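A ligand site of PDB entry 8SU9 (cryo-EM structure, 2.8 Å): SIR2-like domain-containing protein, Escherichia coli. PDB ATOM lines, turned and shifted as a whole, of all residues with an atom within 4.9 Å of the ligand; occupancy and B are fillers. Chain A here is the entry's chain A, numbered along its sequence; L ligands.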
ATOM      1  N   GLY A  33      21.011 -10.389   1.395  1.00  0.00           N
ATOM      2  CA  GLY A  33      21.840 -11.561   1.259  1.00  0.00           C
ATOM      3  C   GLY A  33      23.189 -11.256   0.647  1.00  0.00           C
ATOM      4  O   GLY A  33      23.585 -10.099   0.537  1.00  0.00           O
ATOM      5  N   ALA A  34      23.920 -12.305   0.241  1.00  0.00           N
ATOM      6  CA  ALA A  34      25.257 -12.114  -0.302  1.00  0.00           C
ATOM      7  C   ALA A  34      25.244 -11.494  -1.689  1.00  0.00           C
ATOM      8  O   ALA A  34      26.291 -11.049  -2.161  1.00  0.00           O
ATOM      9  CB  ALA A  34      26.010 -13.439  -0.329  1.00  0.00           C
ATOM     10  N   GLY A  35      24.093 -11.465  -2.355  1.00  0.00           N
ATOM     11  CA  GLY A  35      24.009 -10.852  -3.666  1.00  0.00           C
ATOM     12  C   GLY A  35      23.956  -9.343  -3.658  1.00  0.00           C
ATOM     13  O   GLY A  35      24.222  -8.728  -4.700  1.00  0.00           O
ATOM     14  N   VAL A  38      27.544  -7.613  -4.422  1.00  0.00           N
ATOM     15  CA  VAL A  38      28.298  -7.901  -5.635  1.00  0.00           C
ATOM     16  C   VAL A  38      28.673  -6.618  -6.350  1.00  0.00           C
ATOM     17  O   VAL A  38      29.787  -6.483  -6.872  1.00  0.00           O
ATOM     18  CB  VAL A  38      27.487  -8.849  -6.545  1.00  0.00           C
ATOM     19  CG1 VAL A  38      28.100  -8.896  -7.944  1.00  0.00           C
ATOM     20  CG2 VAL A  38      27.427 -10.238  -5.947  1.00  0.00           C
ATOM     21  N   THR A  44      29.855 -14.179  -4.595  1.00  0.00           N
ATOM     22  CA  THR A  44      28.951 -15.156  -4.017  1.00  0.00           C
ATOM     23  C   THR A  44      29.720 -16.398  -3.562  1.00  0.00           C
ATOM     24  O   THR A  44      30.950 -16.455  -3.607  1.00  0.00           O
ATOM     25  CB  THR A  44      27.868 -15.536  -5.032  1.00  0.00           C
ATOM     26  OG1 THR A  44      28.488 -15.986  -6.245  1.00  0.00           O
ATOM     27  CG2 THR A  44      26.992 -14.336  -5.334  1.00  0.00           C
ATOM     28  N   MET A  45      28.967 -17.414  -3.099  1.00  0.00           N
ATOM     29  CA  MET A  45      29.577 -18.624  -2.557  1.00  0.00           C
ATOM     30  C   MET A  45      30.161 -19.516  -3.645  1.00  0.00           C
ATOM     31  O   MET A  45      31.170 -20.195  -3.412  1.00  0.00           O
ATOM     32  CB  MET A  45      28.561 -19.400  -1.731  1.00  0.00           C
ATOM     33  CG  MET A  45      28.153 -18.717  -0.440  1.00  0.00           C
ATOM     34  SD  MET A  45      29.535 -18.495   0.703  1.00  0.00           S
ATOM     35  CE  MET A  45      29.707 -16.710   0.695  1.00  0.00           C
ATOM     36  N   ASN A  81      27.896 -25.855   0.890  1.00  0.00           N
ATOM     37  CA  ASN A  81      27.630 -24.857   1.932  1.00  0.00           C
ATOM     38  C   ASN A  81      28.916 -24.631   2.710  1.00  0.00           C
ATOM     39  O   ASN A  81      29.431 -25.544   3.369  1.00  0.00           O
ATOM     40  CB  ASN A  81      26.509 -25.336   2.851  1.00  0.00           C
ATOM     41  CG  ASN A  81      25.860 -24.215   3.616  1.00  0.00           C
ATOM     42  OD1 ASN A  81      26.534 -23.308   4.109  1.00  0.00           O
ATOM     43  ND2 ASN A  81      24.534 -24.249   3.729  1.00  0.00           N
ATOM     44  N   GLU A  83      29.791 -22.199   5.219  1.00  0.00           N
ATOM     45  CA  GLU A  83      29.731 -21.953   6.660  1.00  0.00           C
ATOM     46  C   GLU A  83      29.284 -23.186   7.442  1.00  0.00           C
ATOM     47  O   GLU A  83      29.496 -23.248   8.656  1.00  0.00           O
ATOM     48  CB  GLU A  83      28.817 -20.780   6.965  1.00  0.00           C
ATOM     49  CG  GLU A  83      27.393 -20.943   6.463  1.00  0.00           C
ATOM     50  CD  GLU A  83      27.201 -20.345   5.092  1.00  0.00           C
ATOM     51  OE1 GLU A  83      28.211 -20.124   4.385  1.00  0.00           O
ATOM     52  OE2 GLU A  83      26.039 -20.112   4.714  1.00  0.00           O
ATOM     53  N   THR A 167      22.786 -11.336   6.189  1.00  0.00           N
ATOM     54  CA  THR A 167      23.593 -12.532   6.379  1.00  0.00           C
ATOM     55  C   THR A 167      25.054 -12.313   5.989  1.00  0.00           C
ATOM     56  O   THR A 167      25.806 -13.277   5.870  1.00  0.00           O
ATOM     57  CB  THR A 167      23.023 -13.710   5.579  1.00  0.00           C
ATOM     58  OG1 THR A 167      23.122 -13.431   4.177  1.00  0.00           O
ATOM     59  CG2 THR A 167      21.563 -13.933   5.941  1.00  0.00           C
ATOM     60  N   HIS A 227      25.267 -13.769  11.153  1.00  0.00           N
ATOM     61  CA  HIS A 227      26.412 -14.666  11.064  1.00  0.00           C
ATOM     62  C   HIS A 227      27.684 -14.049  11.637  1.00  0.00           C
ATOM     63  O   HIS A 227      28.783 -14.488  11.308  1.00  0.00           O
ATOM     64  CB  HIS A 227      26.657 -15.093   9.612  1.00  0.00           C
ATOM     65  CG  HIS A 227      25.704 -16.148   9.131  1.00  0.00           C
ATOM     66  ND1 HIS A 227      25.167 -16.136   7.867  1.00  0.00           N
ATOM     67  CD2 HIS A 227      25.195 -17.239   9.749  1.00  0.00           C
ATOM     68  CE1 HIS A 227      24.368 -17.176   7.721  1.00  0.00           C
ATOM     69  NE2 HIS A 227      24.367 -17.861   8.846  1.00  0.00           N
ATOM     70  N   ASN A 305      15.698  -9.585  -0.781  1.00  0.00           N
ATOM     71  CA  ASN A 305      16.503  -9.357  -1.974  1.00  0.00           C
ATOM     72  C   ASN A 305      17.910  -9.877  -1.721  1.00  0.00           C
ATOM     73  O   ASN A 305      18.515  -9.556  -0.698  1.00  0.00           O
ATOM     74  CB  ASN A 305      16.531  -7.872  -2.332  1.00  0.00           C
ATOM     75  CG  ASN A 305      17.279  -7.598  -3.621  1.00  0.00           C
ATOM     76  OD1 ASN A 305      18.510  -7.555  -3.633  1.00  0.00           O
ATOM     77  ND2 ASN A 305      16.546  -7.420  -4.702  1.00  0.00           N
ATOM     78  N   GLY A 306      18.422 -10.666  -2.658  1.00  0.00           N
ATOM     79  CA  GLY A 306      19.751 -11.241  -2.557  1.00  0.00           C
ATOM     80  C   GLY A 306      19.816 -12.595  -1.887  1.00  0.00           C
ATOM     81  O   GLY A 306      20.889 -13.211  -1.885  1.00  0.00           O
ATOM     82  N   PHE A 307      18.713 -13.083  -1.317  1.00  0.00           N
ATOM     83  CA  PHE A 307      18.712 -14.357  -0.622  1.00  0.00           C
ATOM     84  C   PHE A 307      18.640 -15.513  -1.617  1.00  0.00           C
ATOM     85  O   PHE A 307      18.040 -15.396  -2.680  1.00  0.00           O
ATOM     86  CB  PHE A 307      17.538 -14.426   0.353  1.00  0.00           C
ATOM     87  CG  PHE A 307      17.668 -15.497   1.394  1.00  0.00           C
ATOM     88  CD1 PHE A 307      18.781 -15.558   2.199  1.00  0.00           C
ATOM     89  CD2 PHE A 307      16.674 -16.442   1.552  1.00  0.00           C
ATOM     90  CE1 PHE A 307      18.907 -16.543   3.153  1.00  0.00           C
ATOM     91  CE2 PHE A 307      16.792 -17.437   2.500  1.00  0.00           C
ATOM     92  CZ  PHE A 307      17.914 -17.491   3.298  1.00  0.00           C
ATOM     93  N   GLY A 308      19.267 -16.627  -1.241  1.00  0.00           N
ATOM     94  CA  GLY A 308      19.326 -17.791  -2.121  1.00  0.00           C
ATOM     95  C   GLY A 308      18.358 -18.901  -1.774  1.00  0.00           C
ATOM     96  O   GLY A 308      18.261 -19.884  -2.513  1.00  0.00           O
ATOM     97  N   PHE A 309      17.655 -18.775  -0.652  1.00  0.00           N
ATOM     98  CA  PHE A 309      16.672 -19.758  -0.192  1.00  0.00           C
ATOM     99  C   PHE A 309      17.289 -21.142  -0.014  1.00  0.00           C
ATOM    100  O   PHE A 309      16.641 -22.159  -0.293  1.00  0.00           O
ATOM    101  CB  PHE A 309      15.473 -19.830  -1.129  1.00  0.00           C
ATOM    102  CG  PHE A 309      14.501 -18.713  -0.955  1.00  0.00           C
ATOM    103  CD1 PHE A 309      14.667 -17.515  -1.622  1.00  0.00           C
ATOM    104  CD2 PHE A 309      13.404 -18.859  -0.114  1.00  0.00           C
ATOM    105  CE1 PHE A 309      13.771 -16.483  -1.465  1.00  0.00           C
ATOM    106  CE2 PHE A 309      12.506 -17.818   0.049  1.00  0.00           C
ATOM    107  CZ  PHE A 309      12.696 -16.639  -0.621  1.00  0.00           C
ATOM    108  N   GLY A 310      18.532 -21.213   0.455  1.00  0.00           N
ATOM    109  CA  GLY A 310      19.180 -22.487   0.694  1.00  0.00           C
ATOM    110  C   GLY A 310      19.296 -22.839   2.169  1.00  0.00           C
ATOM    111  O   GLY A 310      20.066 -23.732   2.535  1.00  0.00           O
ATOM    112  N   ASP A 311      18.548 -22.143   3.017  1.00  0.00           N
ATOM    113  CA  ASP A 311      18.588 -22.347   4.456  1.00  0.00           C
ATOM    114  C   ASP A 311      17.246 -22.904   4.918  1.00  0.00           C
ATOM    115  O   ASP A 311      16.196 -22.334   4.602  1.00  0.00           O
ATOM    116  CB  ASP A 311      18.904 -21.049   5.194  1.00  0.00           C
ATOM    117  CG  ASP A 311      19.425 -21.272   6.595  1.00  0.00           C
ATOM    118  OD1 ASP A 311      18.785 -22.040   7.351  1.00  0.00           O
ATOM    119  OD2 ASP A 311      20.464 -20.692   6.948  1.00  0.00           O
ATOM    120  N   TYR A 333      13.818 -12.754  -7.249  1.00  0.00           N
ATOM    121  CA  TYR A 333      14.574 -13.946  -7.623  1.00  0.00           C
ATOM    122  C   TYR A 333      15.030 -13.788  -9.072  1.00  0.00           C
ATOM    123  O   TYR A 333      14.204 -13.846 -10.001  1.00  0.00           O
ATOM    124  CB  TYR A 333      13.738 -15.210  -7.444  1.00  0.00           C
ATOM    125  CG  TYR A 333      14.551 -16.488  -7.347  1.00  0.00           C
ATOM    126  CD1 TYR A 333      15.263 -16.790  -6.203  1.00  0.00           C
ATOM    127  CD2 TYR A 333      14.586 -17.382  -8.404  1.00  0.00           C
ATOM    128  CE1 TYR A 333      15.995 -17.950  -6.101  1.00  0.00           C
ATOM    129  CE2 TYR A 333      15.329 -18.548  -8.308  1.00  0.00           C
ATOM    130  CZ  TYR A 333      16.028 -18.830  -7.161  1.00  0.00           C
ATOM    131  OH  TYR A 333      16.759 -19.987  -7.082  1.00  0.00           O
ATOM    132  N   PRO A 334      16.326 -13.571  -9.312  1.00  0.00           N
ATOM    133  CA  PRO A 334      16.783 -13.252 -10.674  1.00  0.00           C
ATOM    134  C   PRO A 334      16.460 -14.308 -11.721  1.00  0.00           C
ATOM    135  O   PRO A 334      16.105 -13.957 -12.855  1.00  0.00           O
ATOM    136  CB  PRO A 334      18.291 -13.067 -10.496  1.00  0.00           C
ATOM    137  CG  PRO A 334      18.464 -12.704  -9.070  1.00  0.00           C
ATOM    138  CD  PRO A 334      17.422 -13.495  -8.337  1.00  0.00           C
ATOM    139  N   GLU A 335      16.569 -15.591 -11.384  1.00  0.00           N
ATOM    140  CA  GLU A 335      16.411 -16.665 -12.362  1.00  0.00           C
ATOM    141  C   GLU A 335      15.208 -17.536 -11.997  1.00  0.00           C
ATOM    142  O   GLU A 335      15.319 -18.580 -11.350  1.00  0.00           O
ATOM    143  CB  GLU A 335      17.755 -17.475 -12.485  1.00  0.00           C
ATOM    144  CG  GLU A 335      18.208 -18.212 -11.236  1.00  0.00           C
ATOM    145  CD  GLU A 335      19.541 -18.896 -11.417  1.00  0.00           C
ATOM    146  OE1 GLU A 335      20.120 -18.783 -12.508  1.00  0.00           O
ATOM    147  OE2 GLU A 335      20.007 -19.568 -10.466  1.00  0.00           O
ATOM    148  N   ALA A 375      15.585  -7.887 -11.465  1.00  0.00           N
ATOM    149  CA  ALA A 375      15.433  -8.263 -10.064  1.00  0.00           C
ATOM    150  C   ALA A 375      16.707  -8.028  -9.266  1.00  0.00           C
ATOM    151  O   ALA A 375      16.836  -8.531  -8.152  1.00  0.00           O
ATOM    152  CB  ALA A 375      14.999  -9.725  -9.953  1.00  0.00           C
ATOM    153  N   TYR A 376      17.637  -7.258  -9.807  1.00  0.00           N
ATOM    154  CA  TYR A 376      18.908  -6.990  -9.144  1.00  0.00           C
ATOM    155  C   TYR A 376      18.731  -5.927  -8.066  1.00  0.00           C
ATOM    156  O   TYR A 376      17.666  -5.318  -7.915  1.00  0.00           O
ATOM    157  CB  TYR A 376      19.957  -6.556 -10.160  1.00  0.00           C
ATOM    158  CG  TYR A 376      20.662  -7.716 -10.836  1.00  0.00           C
ATOM    159  CD1 TYR A 376      20.260  -9.023 -10.621  1.00  0.00           C
ATOM    160  CD2 TYR A 376      21.747  -7.499 -11.675  1.00  0.00           C
ATOM    161  CE1 TYR A 376      20.905 -10.080 -11.232  1.00  0.00           C
ATOM    162  CE2 TYR A 376      22.391  -8.551 -12.294  1.00  0.00           C
ATOM    163  CZ  TYR A 376      21.964  -9.837 -12.063  1.00  0.00           C
ATOM    164  OH  TYR A 376      22.616 -10.878 -12.676  1.00  0.00           O
ATOM    165  N   PHE A 377      19.796  -5.711  -7.297  1.00  0.00           N
ATOM    166  CA  PHE A 377      19.744  -4.785  -6.167  1.00  0.00           C
ATOM    167  C   PHE A 377      19.509  -3.350  -6.629  1.00  0.00           C
ATOM    168  O   PHE A 377      18.736  -2.606  -6.014  1.00  0.00           O
ATOM    169  CB  PHE A 377      21.024  -4.873  -5.349  1.00  0.00           C
ATOM    170  CG  PHE A 377      21.003  -4.082  -4.072  1.00  0.00           C
ATOM    171  CD1 PHE A 377      20.092  -4.379  -3.073  1.00  0.00           C
ATOM    172  CD2 PHE A 377      21.880  -3.035  -3.880  1.00  0.00           C
ATOM    173  CE1 PHE A 377      20.074  -3.650  -1.900  1.00  0.00           C
ATOM    174  CE2 PHE A 377      21.862  -2.306  -2.707  1.00  0.00           C
ATOM    175  CZ  PHE A 377      20.955  -2.619  -1.720  1.00  0.00           C
HETATM  176  N1  LIG L   1      21.747  -8.773  -7.228  1.00  0.00           N
HETATM  177  C1  LIG L   1      20.875  -9.537  -6.592  1.00  0.00           C
HETATM  178  N2  LIG L   1      20.882 -10.854  -6.463  1.00  0.00           N
HETATM  179  C2  LIG L   1      21.935 -11.402  -7.071  1.00  0.00           C
HETATM  180  C3  LIG L   1      22.917 -10.739  -7.763  1.00  0.00           C
HETATM  181  C4  LIG L   1      22.793  -9.337  -7.833  1.00  0.00           C
HETATM  182  N3  LIG L   1      23.674  -8.565  -8.478  1.00  0.00           N
HETATM  183  N4  LIG L   1      23.843 -11.616  -8.255  1.00  0.00           N
HETATM  184  C5  LIG L   1      23.424 -12.791  -7.862  1.00  0.00           C
HETATM  185  N5  LIG L   1      22.270 -12.719  -7.134  1.00  0.00           N
HETATM  186  P1  LIG L   1      24.282 -17.081  -2.302  1.00  0.00           P
HETATM  187  P2  LIG L   1      22.852 -16.130   0.034  1.00  0.00           P
HETATM  188  C6  LIG L   1      21.528 -13.812  -6.542  1.00  0.00           C
HETATM  189  O1  LIG L   1      24.755 -18.372  -2.873  1.00  0.00           O
HETATM  190  O2  LIG L   1      21.485 -16.538   0.455  1.00  0.00           O
HETATM  191  C7  LIG L   1      23.033 -20.334   3.556  1.00  0.00           C
HETATM  192  O3  LIG L   1      21.817 -20.968   3.391  1.00  0.00           O
HETATM  193  C8  LIG L   1      21.822 -15.179  -7.159  1.00  0.00           C
HETATM  194  O4  LIG L   1      21.117 -15.316  -8.363  1.00  0.00           O
HETATM  195  O5  LIG L   1      25.235 -15.929  -2.204  1.00  0.00           O
HETATM  196  O6  LIG L   1      23.066 -14.797  -0.618  1.00  0.00           O
HETATM  197  C9  LIG L   1      22.912 -19.247   4.632  1.00  0.00           C
HETATM  198  O7  LIG L   1      21.589 -18.848   4.836  1.00  0.00           O
HETATM  199  C10 LIG L   1      21.343 -16.091  -6.032  1.00  0.00           C
HETATM  200  O8  LIG L   1      19.943 -16.162  -6.010  1.00  0.00           O
HETATM  201  O9  LIG L   1      23.516 -17.318  -0.876  1.00  0.00           O
HETATM  202  C11 LIG L   1      23.674 -18.088   3.987  1.00  0.00           C
HETATM  203  O10 LIG L   1      23.308 -16.806   4.407  1.00  0.00           O
HETATM  204  C12 LIG L   1      21.812 -15.311  -4.801  1.00  0.00           C
HETATM  205  O11 LIG L   1      21.914 -13.947  -5.213  1.00  0.00           O
HETATM  206  C13 LIG L   1      23.360 -18.286   2.518  1.00  0.00           C
HETATM  207  O12 LIG L   1      23.419 -19.692   2.349  1.00  0.00           O
HETATM  208  C14 LIG L   1      23.133 -15.832  -4.272  1.00  0.00           C
HETATM  209  O13 LIG L   1      22.928 -16.579  -3.096  1.00  0.00           O
HETATM  210  C15 LIG L   1      24.342 -17.598   1.599  1.00  0.00           C
HETATM  211  O14 LIG L   1      23.884 -16.296   1.300  1.00  0.00           O
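OD1 of Asn 81 sits close to OE2 of Glu 83, 3.3 Å away. The backbone NH (N) of Gly 33 sits at hydrogen-bond distance from the backbone carbonyl oxygen (O) of Asn 305 (3.4 Å).
Residues that only touch the ligand: Gly 33 (3.8 Å), Gly 35 (3.5 Å), Thr 44 (3.9 Å), Glu 83 (3.2 Å), His 227 (3.5 Å), Phe 307 (3.4 Å), Pro 334 (3.8 Å), Tyr 376 (3.7 Å) and Phe 377 (3.6 Å). Hydrophobic or aromatic side chains that line the ligand: Ala 34, His 227, Phe 307, Pro 334 and Tyr 376. Along chain A the residues within 4 Å of the ligand span positions 33 to 377. The nearest printed residue that does not touch the ligand is Met 45 (4.1 Å).
The backbone NH (N) of Ala 34 is in hydrogen-bond range of an oxygen (O6) of the ligand (2.8 Å). The backbone NH (N) of Gly 308 is in hydrogen-bond range of an oxygen (O2) of the ligand (2.8 Å). The backbone carbonyl oxygen (O) of Gly 306 sits close to an oxygen (O6) of the ligand (3.0 Å). N of Asp 311 sits close to O3 of the ligand, at 3.5 Å. An oxygen (O7) of the ligand lies within hydrogen-bond range of the side-chain carboxylate of Asp 311 (3.0 Å). An oxygen (O10) of the ligand lies close to the side-chain hydroxyl (OG1) of Thr 167 (3.4 Å). O of Gly 310 lies close to O3 of the ligand (3.4 Å).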
